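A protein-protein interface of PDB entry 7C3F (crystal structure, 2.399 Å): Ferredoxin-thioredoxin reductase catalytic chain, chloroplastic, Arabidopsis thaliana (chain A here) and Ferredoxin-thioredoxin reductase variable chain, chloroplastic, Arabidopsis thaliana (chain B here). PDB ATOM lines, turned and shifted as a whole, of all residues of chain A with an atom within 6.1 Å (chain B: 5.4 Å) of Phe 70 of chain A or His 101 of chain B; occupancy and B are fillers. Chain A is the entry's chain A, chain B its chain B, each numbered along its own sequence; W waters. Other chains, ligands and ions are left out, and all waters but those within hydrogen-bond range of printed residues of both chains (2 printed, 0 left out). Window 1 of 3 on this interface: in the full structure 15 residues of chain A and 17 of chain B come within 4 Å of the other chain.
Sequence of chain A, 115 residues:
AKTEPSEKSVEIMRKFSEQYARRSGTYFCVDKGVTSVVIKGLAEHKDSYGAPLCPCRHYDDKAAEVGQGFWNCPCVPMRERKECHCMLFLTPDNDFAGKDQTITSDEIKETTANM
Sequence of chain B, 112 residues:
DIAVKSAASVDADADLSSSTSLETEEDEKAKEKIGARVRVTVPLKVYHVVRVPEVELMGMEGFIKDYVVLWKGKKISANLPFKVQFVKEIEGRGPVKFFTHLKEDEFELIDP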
ATOM      1  N   GLU A  65      15.836 -25.330  34.929  1.00  0.00           N
ATOM      2  CA  GLU A  65      16.589 -24.114  34.640  1.00  0.00           C
ATOM      3  C   GLU A  65      18.043 -24.259  35.070  1.00  0.00           C
ATOM      4  O   GLU A  65      18.963 -23.887  34.331  1.00  0.00           O
ATOM      5  CB  GLU A  65      15.938 -22.915  35.330  1.00  0.00           C
ATOM      6  CG  GLU A  65      14.532 -22.605  34.852  1.00  0.00           C
ATOM      7  CD  GLU A  65      14.516 -21.764  33.594  1.00  0.00           C
ATOM      8  OE1 GLU A  65      13.411 -21.450  33.102  1.00  0.00           O
ATOM      9  OE2 GLU A  65      15.609 -21.418  33.100  1.00  0.00           O
ATOM     10  N   VAL A  66      18.267 -24.798  36.271  1.00  0.00           N
ATOM     11  CA  VAL A  66      19.628 -25.030  36.746  1.00  0.00           C
ATOM     12  C   VAL A  66      20.355 -26.001  35.822  1.00  0.00           C
ATOM     13  O   VAL A  66      21.547 -25.833  35.530  1.00  0.00           O
ATOM     14  CB  VAL A  66      19.600 -25.537  38.200  1.00  0.00           C
ATOM     15  CG1 VAL A  66      20.902 -26.247  38.556  1.00  0.00           C
ATOM     16  CG2 VAL A  66      19.340 -24.384  39.155  1.00  0.00           C
ATOM     17  N   GLN A  68      19.777 -26.691  32.485  1.00  0.00           N
ATOM     18  CA  GLN A  68      20.109 -26.077  31.204  1.00  0.00           C
ATOM     19  C   GLN A  68      21.165 -24.989  31.369  1.00  0.00           C
ATOM     20  O   GLN A  68      22.101 -24.899  30.565  1.00  0.00           O
ATOM     21  CB  GLN A  68      18.848 -25.518  30.545  1.00  0.00           C
ATOM     22  CG  GLN A  68      18.939 -25.386  29.031  1.00  0.00           C
ATOM     23  CD  GLN A  68      19.665 -24.127  28.588  1.00  0.00           C
ATOM     24  OE1 GLN A  68      19.928 -23.233  29.391  1.00  0.00           O
ATOM     25  NE2 GLN A  68      19.993 -24.055  27.305  1.00  0.00           N
ATOM     26  N   GLY A  69      21.030 -24.147  32.394  1.00  0.00           N
ATOM     27  CA  GLY A  69      22.068 -23.203  32.752  1.00  0.00           C
ATOM     28  C   GLY A  69      21.907 -21.799  32.210  1.00  0.00           C
ATOM     29  O   GLY A  69      22.729 -20.937  32.540  1.00  0.00           O
ATOM     30  N   PHE A  70      20.890 -21.545  31.381  1.00  0.00           N
ATOM     31  CA  PHE A  70      20.714 -20.221  30.786  1.00  0.00           C
ATOM     32  C   PHE A  70      20.689 -19.121  31.841  1.00  0.00           C
ATOM     33  O   PHE A  70      21.326 -18.075  31.673  1.00  0.00           O
ATOM     34  CB  PHE A  70      19.428 -20.188  29.958  1.00  0.00           C
ATOM     35  CG  PHE A  70      19.278 -18.957  29.099  1.00  0.00           C
ATOM     36  CD1 PHE A  70      18.787 -17.774  29.631  1.00  0.00           C
ATOM     37  CD2 PHE A  70      19.603 -18.994  27.754  1.00  0.00           C
ATOM     38  CE1 PHE A  70      18.637 -16.645  28.840  1.00  0.00           C
ATOM     39  CE2 PHE A  70      19.455 -17.871  26.957  1.00  0.00           C
ATOM     40  CZ  PHE A  70      18.972 -16.694  27.501  1.00  0.00           C
ATOM     41  N   TRP A  71      19.957 -19.333  32.934  1.00  0.00           N
ATOM     42  CA  TRP A  71      19.779 -18.310  33.955  1.00  0.00           C
ATOM     43  C   TRP A  71      20.639 -18.539  35.190  1.00  0.00           C
ATOM     44  O   TRP A  71      20.394 -17.911  36.224  1.00  0.00           O
ATOM     45  CB  TRP A  71      18.302 -18.212  34.351  1.00  0.00           C
ATOM     46  CG  TRP A  71      17.473 -17.507  33.321  1.00  0.00           C
ATOM     47  CD1 TRP A  71      16.475 -18.045  32.564  1.00  0.00           C
ATOM     48  CD2 TRP A  71      17.585 -16.135  32.922  1.00  0.00           C
ATOM     49  NE1 TRP A  71      15.953 -17.094  31.723  1.00  0.00           N
ATOM     50  CE2 TRP A  71      16.617 -15.912  31.922  1.00  0.00           C
ATOM     51  CE3 TRP A  71      18.405 -15.072  33.316  1.00  0.00           C
ATOM     52  CZ2 TRP A  71      16.449 -14.672  31.310  1.00  0.00           C
ATOM     53  CZ3 TRP A  71      18.235 -13.840  32.706  1.00  0.00           C
ATOM     54  CH2 TRP A  71      17.265 -13.651  31.715  1.00  0.00           C
ATOM     55  N   ASN A  72      21.632 -19.421  35.116  1.00  0.00           N
ATOM     56  CA  ASN A  72      22.609 -19.532  36.188  1.00  0.00           C
ATOM     57  C   ASN A  72      23.583 -18.365  36.074  1.00  0.00           C
ATOM     58  O   ASN A  72      24.161 -18.133  35.008  1.00  0.00           O
ATOM     59  CB  ASN A  72      23.355 -20.863  36.111  1.00  0.00           C
ATOM     60  CG  ASN A  72      22.477 -22.064  36.453  1.00  0.00           C
ATOM     61  OD1 ASN A  72      21.380 -21.919  37.001  1.00  0.00           O
ATOM     62  ND2 ASN A  72      22.962 -23.258  36.135  1.00  0.00           N
ATOM     63  N   CYS A  73      23.765 -17.637  37.168  1.00  0.00           N
ATOM     64  CA  CYS A  73      24.537 -16.410  37.119  1.00  0.00           C
ATOM     65  C   CYS A  73      26.023 -16.725  36.944  1.00  0.00           C
ATOM     66  O   CYS A  73      26.559 -17.591  37.635  1.00  0.00           O
ATOM     67  CB  CYS A  73      24.309 -15.628  38.419  1.00  0.00           C
ATOM     68  SG  CYS A  73      25.228 -14.103  38.666  1.00  0.00           S
ATOM     69  N   PRO A  74      26.728 -16.019  36.041  1.00  0.00           N
ATOM     70  CA  PRO A  74      26.201 -15.010  35.112  1.00  0.00           C
ATOM     71  C   PRO A  74      25.359 -15.599  33.976  1.00  0.00           C
ATOM     72  O   PRO A  74      25.864 -16.419  33.215  1.00  0.00           O
ATOM     73  CB  PRO A  74      27.466 -14.347  34.564  1.00  0.00           C
ATOM     74  CG  PRO A  74      28.531 -15.373  34.713  1.00  0.00           C
ATOM     75  CD  PRO A  74      28.194 -16.148  35.942  1.00  0.00           C
ATOM     76  N   CYS A  75      24.093 -15.179  33.906  1.00  0.00           N
ATOM     77  CA  CYS A  75      23.199 -15.563  32.819  1.00  0.00           C
ATOM     78  C   CYS A  75      23.834 -15.323  31.449  1.00  0.00           C
ATOM     79  O   CYS A  75      24.680 -14.443  31.275  1.00  0.00           O
ATOM     80  CB  CYS A  75      21.877 -14.803  32.928  1.00  0.00           C
ATOM     81  SG  CYS A  75      21.946 -13.052  32.460  1.00  0.00           S
ATOM     82  N   VAL A  76      23.436 -16.146  30.483  1.00  0.00           N
ATOM     83  CA  VAL A  76      23.724 -15.969  29.057  1.00  0.00           C
ATOM     84  C   VAL A  76      23.630 -14.507  28.612  1.00  0.00           C
ATOM     85  O   VAL A  76      24.574 -14.016  27.973  1.00  0.00           O
ATOM     86  CB  VAL A  76      22.811 -16.876  28.208  1.00  0.00           C
ATOM     87  CG1 VAL A  76      22.735 -16.383  26.776  1.00  0.00           C
ATOM     88  CG2 VAL A  76      23.293 -18.317  28.269  1.00  0.00           C
ATOM     89  N   PRO A  77      22.537 -13.774  28.879  1.00  0.00           N
ATOM     90  CA  PRO A  77      22.505 -12.363  28.449  1.00  0.00           C
ATOM     91  C   PRO A  77      23.622 -11.514  29.030  1.00  0.00           C
ATOM     92  O   PRO A  77      24.098 -10.588  28.360  1.00  0.00           O
ATOM     93  CB  PRO A  77      21.129 -11.883  28.932  1.00  0.00           C
ATOM     94  CG  PRO A  77      20.299 -13.108  28.920  1.00  0.00           C
ATOM     95  CD  PRO A  77      21.216 -14.204  29.379  1.00  0.00           C
ATOM     96  N   ARG A  79      26.698 -12.762  30.038  1.00  0.00           N
ATOM     97  CA  ARG A  79      27.945 -13.249  29.461  1.00  0.00           C
ATOM     98  C   ARG A  79      28.108 -12.782  28.021  1.00  0.00           C
ATOM     99  O   ARG A  79      29.215 -12.431  27.596  1.00  0.00           O
ATOM    100  CB  ARG A  79      27.999 -14.772  29.537  1.00  0.00           C
ATOM    101  CG  ARG A  79      28.278 -15.304  30.925  1.00  0.00           C
ATOM    102  CD  ARG A  79      28.817 -16.711  30.851  1.00  0.00           C
ATOM    103  NE  ARG A  79      27.754 -17.669  30.574  1.00  0.00           N
ATOM    104  CZ  ARG A  79      27.480 -18.715  31.344  1.00  0.00           C
ATOM    105  NH1 ARG A  79      26.492 -19.540  31.022  1.00  0.00           N
ATOM    106  NH2 ARG A  79      28.199 -18.937  32.436  1.00  0.00           N
ATOM    107  N   GLU A  80      27.021 -12.765  27.259  1.00  0.00           N
ATOM    108  CA  GLU A  80      27.128 -12.458  25.841  1.00  0.00           C
ATOM    109  C   GLU A  80      26.936 -10.975  25.553  1.00  0.00           C
ATOM    110  O   GLU A  80      27.694 -10.405  24.766  1.00  0.00           O
ATOM    111  CB  GLU A  80      26.118 -13.295  25.045  1.00  0.00           C
ATOM    112  CG  GLU A  80      26.430 -14.791  25.059  1.00  0.00           C
ATOM    113  CD  GLU A  80      25.480 -15.613  24.202  1.00  0.00           C
ATOM    114  OE1 GLU A  80      24.725 -15.022  23.403  1.00  0.00           O
ATOM    115  OE2 GLU A  80      25.491 -16.853  24.331  1.00  0.00           O
ATOM    116  N   ARG A  81      25.961 -10.325  26.184  1.00  0.00           N
ATOM    117  CA  ARG A  81      25.639  -8.942  25.859  1.00  0.00           C
ATOM    118  C   ARG A  81      25.913  -7.961  26.992  1.00  0.00           C
ATOM    119  O   ARG A  81      25.612  -6.773  26.840  1.00  0.00           O
ATOM    120  CB  ARG A  81      24.171  -8.835  25.435  1.00  0.00           C
ATOM    121  CG  ARG A  81      23.790  -9.821  24.352  1.00  0.00           C
ATOM    122  CD  ARG A  81      22.373  -9.605  23.858  1.00  0.00           C
ATOM    123  NE  ARG A  81      21.948 -10.710  23.007  1.00  0.00           N
ATOM    124  CZ  ARG A  81      20.950 -10.643  22.135  1.00  0.00           C
ATOM    125  NH1 ARG A  81      20.266  -9.517  21.992  1.00  0.00           N
ATOM    126  NH2 ARG A  81      20.637 -11.704  21.402  1.00  0.00           N
ATOM    127  N   VAL B  68      16.827 -23.535  22.455  1.00  0.00           N
ATOM    128  CA  VAL B  68      17.188 -23.943  23.812  1.00  0.00           C
ATOM    129  C   VAL B  68      16.035 -23.852  24.796  1.00  0.00           C
ATOM    130  O   VAL B  68      16.209 -24.204  25.969  1.00  0.00           O
ATOM    131  CB  VAL B  68      18.365 -23.096  24.338  1.00  0.00           C
ATOM    132  CG1 VAL B  68      19.492 -23.059  23.313  1.00  0.00           C
ATOM    133  CG2 VAL B  68      17.901 -21.691  24.677  1.00  0.00           C
ATOM    134  N   ILE B  76      12.358 -24.409  29.265  1.00  0.00           N
ATOM    135  CA  ILE B  76      13.216 -23.426  29.910  1.00  0.00           C
ATOM    136  C   ILE B  76      12.718 -22.048  29.499  1.00  0.00           C
ATOM    137  O   ILE B  76      12.278 -21.857  28.360  1.00  0.00           O
ATOM    138  CB  ILE B  76      14.695 -23.632  29.512  1.00  0.00           C
ATOM    139  CG1 ILE B  76      15.196 -24.979  30.028  1.00  0.00           C
ATOM    140  CG2 ILE B  76      15.577 -22.514  30.040  1.00  0.00           C
ATOM    141  CD1 ILE B  76      14.968 -25.179  31.504  1.00  0.00           C
ATOM    142  N   SER B  77      12.784 -21.092  30.423  1.00  0.00           N
ATOM    143  CA  SER B  77      12.292 -19.739  30.163  1.00  0.00           C
ATOM    144  C   SER B  77      13.419 -18.829  29.673  1.00  0.00           C
ATOM    145  O   SER B  77      13.722 -17.790  30.259  1.00  0.00           O
ATOM    146  CB  SER B  77      11.630 -19.174  31.415  1.00  0.00           C
ATOM    147  OG  SER B  77      12.567 -19.054  32.472  1.00  0.00           O
ATOM    148  N   ALA B  78      14.030 -19.224  28.561  1.00  0.00           N
ATOM    149  CA  ALA B  78      15.129 -18.451  28.004  1.00  0.00           C
ATOM    150  C   ALA B  78      14.579 -17.339  27.120  1.00  0.00           C
ATOM    151  O   ALA B  78      13.753 -17.588  26.237  1.00  0.00           O
ATOM    152  CB  ALA B  78      16.067 -19.355  27.205  1.00  0.00           C
ATOM    153  N   ASN B  79      15.032 -16.109  27.363  1.00  0.00           N
ATOM    154  CA  ASN B  79      14.556 -14.972  26.584  1.00  0.00           C
ATOM    155  C   ASN B  79      15.276 -14.830  25.248  1.00  0.00           C
ATOM    156  O   ASN B  79      14.801 -14.083  24.386  1.00  0.00           O
ATOM    157  CB  ASN B  79      14.658 -13.674  27.402  1.00  0.00           C
ATOM    158  CG  ASN B  79      16.030 -13.456  28.005  1.00  0.00           C
ATOM    159  OD1 ASN B  79      16.956 -14.230  27.775  1.00  0.00           O
ATOM    160  ND2 ASN B  79      16.163 -12.399  28.797  1.00  0.00           N
ATOM    161  N   LEU B  80      16.413 -15.504  25.066  1.00  0.00           N
ATOM    162  CA  LEU B  80      17.139 -15.552  23.797  1.00  0.00           C
ATOM    163  C   LEU B  80      17.205 -17.018  23.383  1.00  0.00           C
ATOM    164  O   LEU B  80      18.220 -17.696  23.598  1.00  0.00           O
ATOM    165  CB  LEU B  80      18.532 -14.935  23.920  1.00  0.00           C
ATOM    166  CG  LEU B  80      18.611 -13.541  24.545  1.00  0.00           C
ATOM    167  CD1 LEU B  80      20.025 -13.259  25.024  1.00  0.00           C
ATOM    168  CD2 LEU B  80      18.159 -12.480  23.558  1.00  0.00           C
ATOM    169  N   PRO B  81      16.129 -17.548  22.793  1.00  0.00           N
ATOM    170  CA  PRO B  81      15.988 -19.009  22.696  1.00  0.00           C
ATOM    171  C   PRO B  81      16.800 -19.678  21.596  1.00  0.00           C
ATOM    172  O   PRO B  81      17.001 -20.897  21.671  1.00  0.00           O
ATOM    173  CB  PRO B  81      14.486 -19.192  22.449  1.00  0.00           C
ATOM    174  CG  PRO B  81      14.082 -17.950  21.726  1.00  0.00           C
ATOM    175  CD  PRO B  81      14.963 -16.836  22.240  1.00  0.00           C
ATOM    176  N   PHE B  82      17.267 -18.951  20.585  1.00  0.00           N
ATOM    177  CA  PHE B  82      17.928 -19.563  19.433  1.00  0.00           C
ATOM    178  C   PHE B  82      19.440 -19.474  19.589  1.00  0.00           C
ATOM    179  O   PHE B  82      20.025 -18.395  19.459  1.00  0.00           O
ATOM    180  CB  PHE B  82      17.472 -18.906  18.134  1.00  0.00           C
ATOM    181  CG  PHE B  82      16.051 -19.199  17.796  1.00  0.00           C
ATOM    182  CD1 PHE B  82      15.685 -20.440  17.302  1.00  0.00           C
ATOM    183  CD2 PHE B  82      15.072 -18.252  18.008  1.00  0.00           C
ATOM    184  CE1 PHE B  82      14.366 -20.720  17.002  1.00  0.00           C
ATOM    185  CE2 PHE B  82      13.754 -18.528  17.714  1.00  0.00           C
ATOM    186  CZ  PHE B  82      13.400 -19.761  17.209  1.00  0.00           C
ATOM    187  N   LYS B  83      20.067 -20.620  19.843  1.00  0.00           N
ATOM    188  CA  LYS B  83      21.520 -20.724  19.891  1.00  0.00           C
ATOM    189  C   LYS B  83      22.034 -20.848  18.461  1.00  0.00           C
ATOM    190  O   LYS B  83      21.779 -21.851  17.788  1.00  0.00           O
ATOM    191  CB  LYS B  83      21.925 -21.923  20.738  1.00  0.00           C
ATOM    192  CG  LYS B  83      23.407 -22.036  21.033  1.00  0.00           C
ATOM    193  CD  LYS B  83      23.696 -23.365  21.710  1.00  0.00           C
ATOM    194  CE  LYS B  83      25.184 -23.631  21.827  1.00  0.00           C
ATOM    195  NZ  LYS B  83      25.459 -24.825  22.676  1.00  0.00           N
ATOM    196  N   VAL B  84      22.753 -19.831  17.992  1.00  0.00           N
ATOM    197  CA  VAL B  84      23.173 -19.729  16.598  1.00  0.00           C
ATOM    198  C   VAL B  84      24.687 -19.861  16.529  1.00  0.00           C
ATOM    199  O   VAL B  84      25.412 -19.192  17.274  1.00  0.00           O
ATOM    200  CB  VAL B  84      22.710 -18.405  15.966  1.00  0.00           C
ATOM    201  CG1 VAL B  84      23.178 -18.314  14.522  1.00  0.00           C
ATOM    202  CG2 VAL B  84      21.203 -18.282  16.048  1.00  0.00           C
ATOM    203  N   PHE B  99      29.165 -19.549  19.548  1.00  0.00           N
ATOM    204  CA  PHE B  99      27.711 -19.504  19.619  1.00  0.00           C
ATOM    205  C   PHE B  99      27.243 -18.219  20.297  1.00  0.00           C
ATOM    206  O   PHE B  99      27.896 -17.708  21.211  1.00  0.00           O
ATOM    207  CB  PHE B  99      27.155 -20.713  20.376  1.00  0.00           C
ATOM    208  CG  PHE B  99      27.617 -22.036  19.836  1.00  0.00           C
ATOM    209  CD1 PHE B  99      27.142 -22.511  18.624  1.00  0.00           C
ATOM    210  CD2 PHE B  99      28.522 -22.809  20.545  1.00  0.00           C
ATOM    211  CE1 PHE B  99      27.565 -23.731  18.127  1.00  0.00           C
ATOM    212  CE2 PHE B  99      28.949 -24.031  20.052  1.00  0.00           C
ATOM    213  CZ  PHE B  99      28.469 -24.490  18.842  1.00  0.00           C
ATOM    214  N   THR B 100      26.089 -17.711  19.850  1.00  0.00           N
ATOM    215  CA  THR B 100      25.394 -16.603  20.499  1.00  0.00           C
ATOM    216  C   THR B 100      23.893 -16.835  20.408  1.00  0.00           C
ATOM    217  O   THR B 100      23.388 -17.270  19.370  1.00  0.00           O
ATOM    218  CB  THR B 100      25.697 -15.233  19.865  1.00  0.00           C
ATOM    219  OG1 THR B 100      25.043 -15.142  18.596  1.00  0.00           O
ATOM    220  CG2 THR B 100      27.187 -15.013  19.669  1.00  0.00           C
ATOM    221  N   HIS B 101      23.184 -16.544  21.494  1.00  0.00           N
ATOM    222  CA  HIS B 101      21.739 -16.722  21.539  1.00  0.00           C
ATOM    223  C   HIS B 101      21.036 -15.479  21.006  1.00  0.00           C
ATOM    224  O   HIS B 101      21.408 -14.350  21.338  1.00  0.00           O
ATOM    225  CB  HIS B 101      21.278 -17.029  22.963  1.00  0.00           C
ATOM    226  CG  HIS B 101      21.873 -18.279  23.531  1.00  0.00           C
ATOM    227  ND1 HIS B 101      23.215 -18.397  23.824  1.00  0.00           N
ATOM    228  CD2 HIS B 101      21.314 -19.470  23.852  1.00  0.00           C
ATOM    229  CE1 HIS B 101      23.455 -19.603  24.308  1.00  0.00           C
ATOM    230  NE2 HIS B 101      22.317 -20.274  24.334  1.00  0.00           N
ATOM    231  N   LEU B 102      20.012 -15.690  20.182  1.00  0.00           N
ATOM    232  CA  LEU B 102      19.308 -14.595  19.529  1.00  0.00           C
ATOM    233  C   LEU B 102      17.802 -14.748  19.672  1.00  0.00           C
ATOM    234  O   LEU B 102      17.280 -15.846  19.882  1.00  0.00           O
ATOM    235  CB  LEU B 102      19.655 -14.502  18.038  1.00  0.00           C
ATOM    236  CG  LEU B 102      21.127 -14.469  17.639  1.00  0.00           C
ATOM    237  CD1 LEU B 102      21.264 -14.445  16.124  1.00  0.00           C
ATOM    238  CD2 LEU B 102      21.825 -13.272  18.261  1.00  0.00           C
ATOM    239  N   LYS B 103      17.114 -13.618  19.535  1.00  0.00           N
ATOM    240  CA  LYS B 103      15.663 -13.569  19.434  1.00  0.00           C
ATOM    241  C   LYS B 103      15.209 -13.561  17.983  1.00  0.00           C
ATOM    242  O   LYS B 103      15.976 -13.271  17.059  1.00  0.00           O
ATOM    243  CB  LYS B 103      15.092 -12.342  20.141  1.00  0.00           C
ATOM    244  CG  LYS B 103      14.964 -12.493  21.627  1.00  0.00           C
ATOM    245  CD  LYS B 103      15.143 -11.145  22.276  1.00  0.00           C
ATOM    246  CE  LYS B 103      14.376 -10.075  21.519  1.00  0.00           C
ATOM    247  NZ  LYS B 103      14.972  -8.727  21.698  1.00  0.00           N
ATOM    248  N   GLU B 106      15.689 -10.545  15.762  1.00  0.00           N
ATOM    249  CA  GLU B 106      17.046 -10.039  15.608  1.00  0.00           C
ATOM    250  C   GLU B 106      17.753 -10.639  14.405  1.00  0.00           C
ATOM    251  O   GLU B 106      18.897 -10.267  14.123  1.00  0.00           O
ATOM    252  CB  GLU B 106      17.868 -10.314  16.874  1.00  0.00           C
ATOM    253  CG  GLU B 106      17.416  -9.542  18.105  1.00  0.00           C
ATOM    254  CD  GLU B 106      18.197  -9.923  19.349  1.00  0.00           C
ATOM    255  OE1 GLU B 106      18.635 -11.088  19.442  1.00  0.00           O
ATOM    256  OE2 GLU B 106      18.371  -9.059  20.237  1.00  0.00           O
HETATM  257  O   HOH W   1      23.219 -13.090  22.945  1.00  0.00           O
HETATM  258  O   HOH W   2      21.931 -22.006  25.984  1.00  0.00           O
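OE1 of Glu 65 of chain A is in hydrogen-bond range of OG of Ser 77 of chain B (2.6 Å). NE1 of Trp 71 of chain A sits at hydrogen-bond distance from O of Ser 77 of chain B. The side-chain carboxylate (OE2) of Glu 80 of chain A is in hydrogen-bond range of a ring nitrogen (ND1) of His 101 of chain B, 2.8 Å away. The guanidinium group (NH2) of Arg 81 of chain A is in hydrogen-bond range of the backbone carbonyl oxygen (O) of His 101 of chain B (2.8 Å). NH1 of Arg 81 of chain A lies within salt-bridge range of OE2 of Glu 106 of chain B.
N of Phe 70 of chain A lies within hydrogen-bond range of OE1 of Gln 68 of chain A. N of Val 76 of chain A is in hydrogen-bond range of O of Phe 70 of chain A (3.1 Å). The backbone NH (N) of Val 68 of chain B lies within hydrogen-bond range of the backbone carbonyl oxygen (O) of Pro 81 of chain B, 2.8 Å away. The backbone NH of Leu 102 of chain B sits at hydrogen-bond distance from the backbone carbonyl oxygen of Phe 82 of chain B, 2.8 Å away. The backbone NH (N) of Val 84 of chain B sits at hydrogen-bond distance from the backbone carbonyl oxygen (O) of Thr 100 of chain B (3.0 Å). The side-chain amino group (NZ) of Lys 103 of chain B lies within salt-bridge range of the side-chain carboxylate (OE2) of Glu 106 of chain B (3.7 Å).
OE2 of Glu 65 of chain A touches CG2 of Ile 76 of chain B, 3.3 Å away. Ile 76 of chain B touches Gln 68 of chain A (CG1 to CB, 3.7 Å). CB of Ala 78 of chain B touches CD2 of Phe 70 of chain A (3.6 Å). Leu 80 of chain B touches Phe 70 of chain A (O to CE2, 3.6 Å). His 101 of chain B touches Phe 70 of chain A (CD2 to CE2, 3.96 Å). CH2 of Trp 71 of chain A touches ND2 of Asn 79 of chain B (3.4 Å). ND1 of His 101 of chain B touches CG1 of Val 76 of chain A, 3.6 Å away. Leu 80 of chain B touches Pro 77 of chain A (CD1 to CG, 3.9 Å). OE1 of Glu 80 of chain A touches CA of Thr 100 of chain B, at 3.4 Å. Arg 81 of chain A touches Leu 102 of chain B.
Of the printed residues of chain B, Gln 68 of chain A touches Val 68 and Ile 76. Phe 70 of chain A touches just these residues of chain B: Ala 78 (3.6 Å), Asn 79 (3.1 Å), Leu 80 (3.6 Å) and His 101 (3.96 Å). Cys 73 of chain A touches none of the printed residues of chain B. Printed residues of chain B within 4 Å of Pro 77 of chain A: Asn 79 and Leu 80. Arg 79 of chain A touches none of the printed residues of chain B. Of the printed residues of chain A, Val 68 of chain B touches Gln 68 (3.5 Å). Of the printed residues of chain A, Thr 100 of chain B touches Glu 80 (3.4 Å). His 101 of chain B touches just these residues of chain A: Phe 70 (3.96 Å), Val 76 (3.6 Å), Glu 80 (2.8 Å) and Arg 81 (2.8 Å). Of the printed residues of chain A, Leu 102 of chain B touches Arg 81 (3.7 Å). The nearest residue of chain B that does not touch Phe 70 of chain A is Val 68 of chain B (4.4 Å). The nearest residue of chain A that does not touch His 101 of chain B is Gln 68 of chain A (5.3 Å).
Of the 15 printed residues of chain A, 8 touch a printed residue of chain B. Printed residues of chain A that touch a printed residue of chain B: Glu 65, Gln 68, Phe 70, Trp 71, Val 76, Pro 77, Glu 80 and Arg 81. Hydrophobic or aromatic side chains of chain A that line the printed part of chain B: Phe 70, Trp 71, Val 76 and Pro 77.
Water W2 lies within hydrogen-bond range of NE2 of His 101 of chain B (2.4 Å) and NE2 of Gln 68 of chain A (3.1 Å). Water W1 lies within hydrogen-bond range of OE1 of Glu 80 of chain A, NE of Arg 81 of chain A and O of His 101 of chain B.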
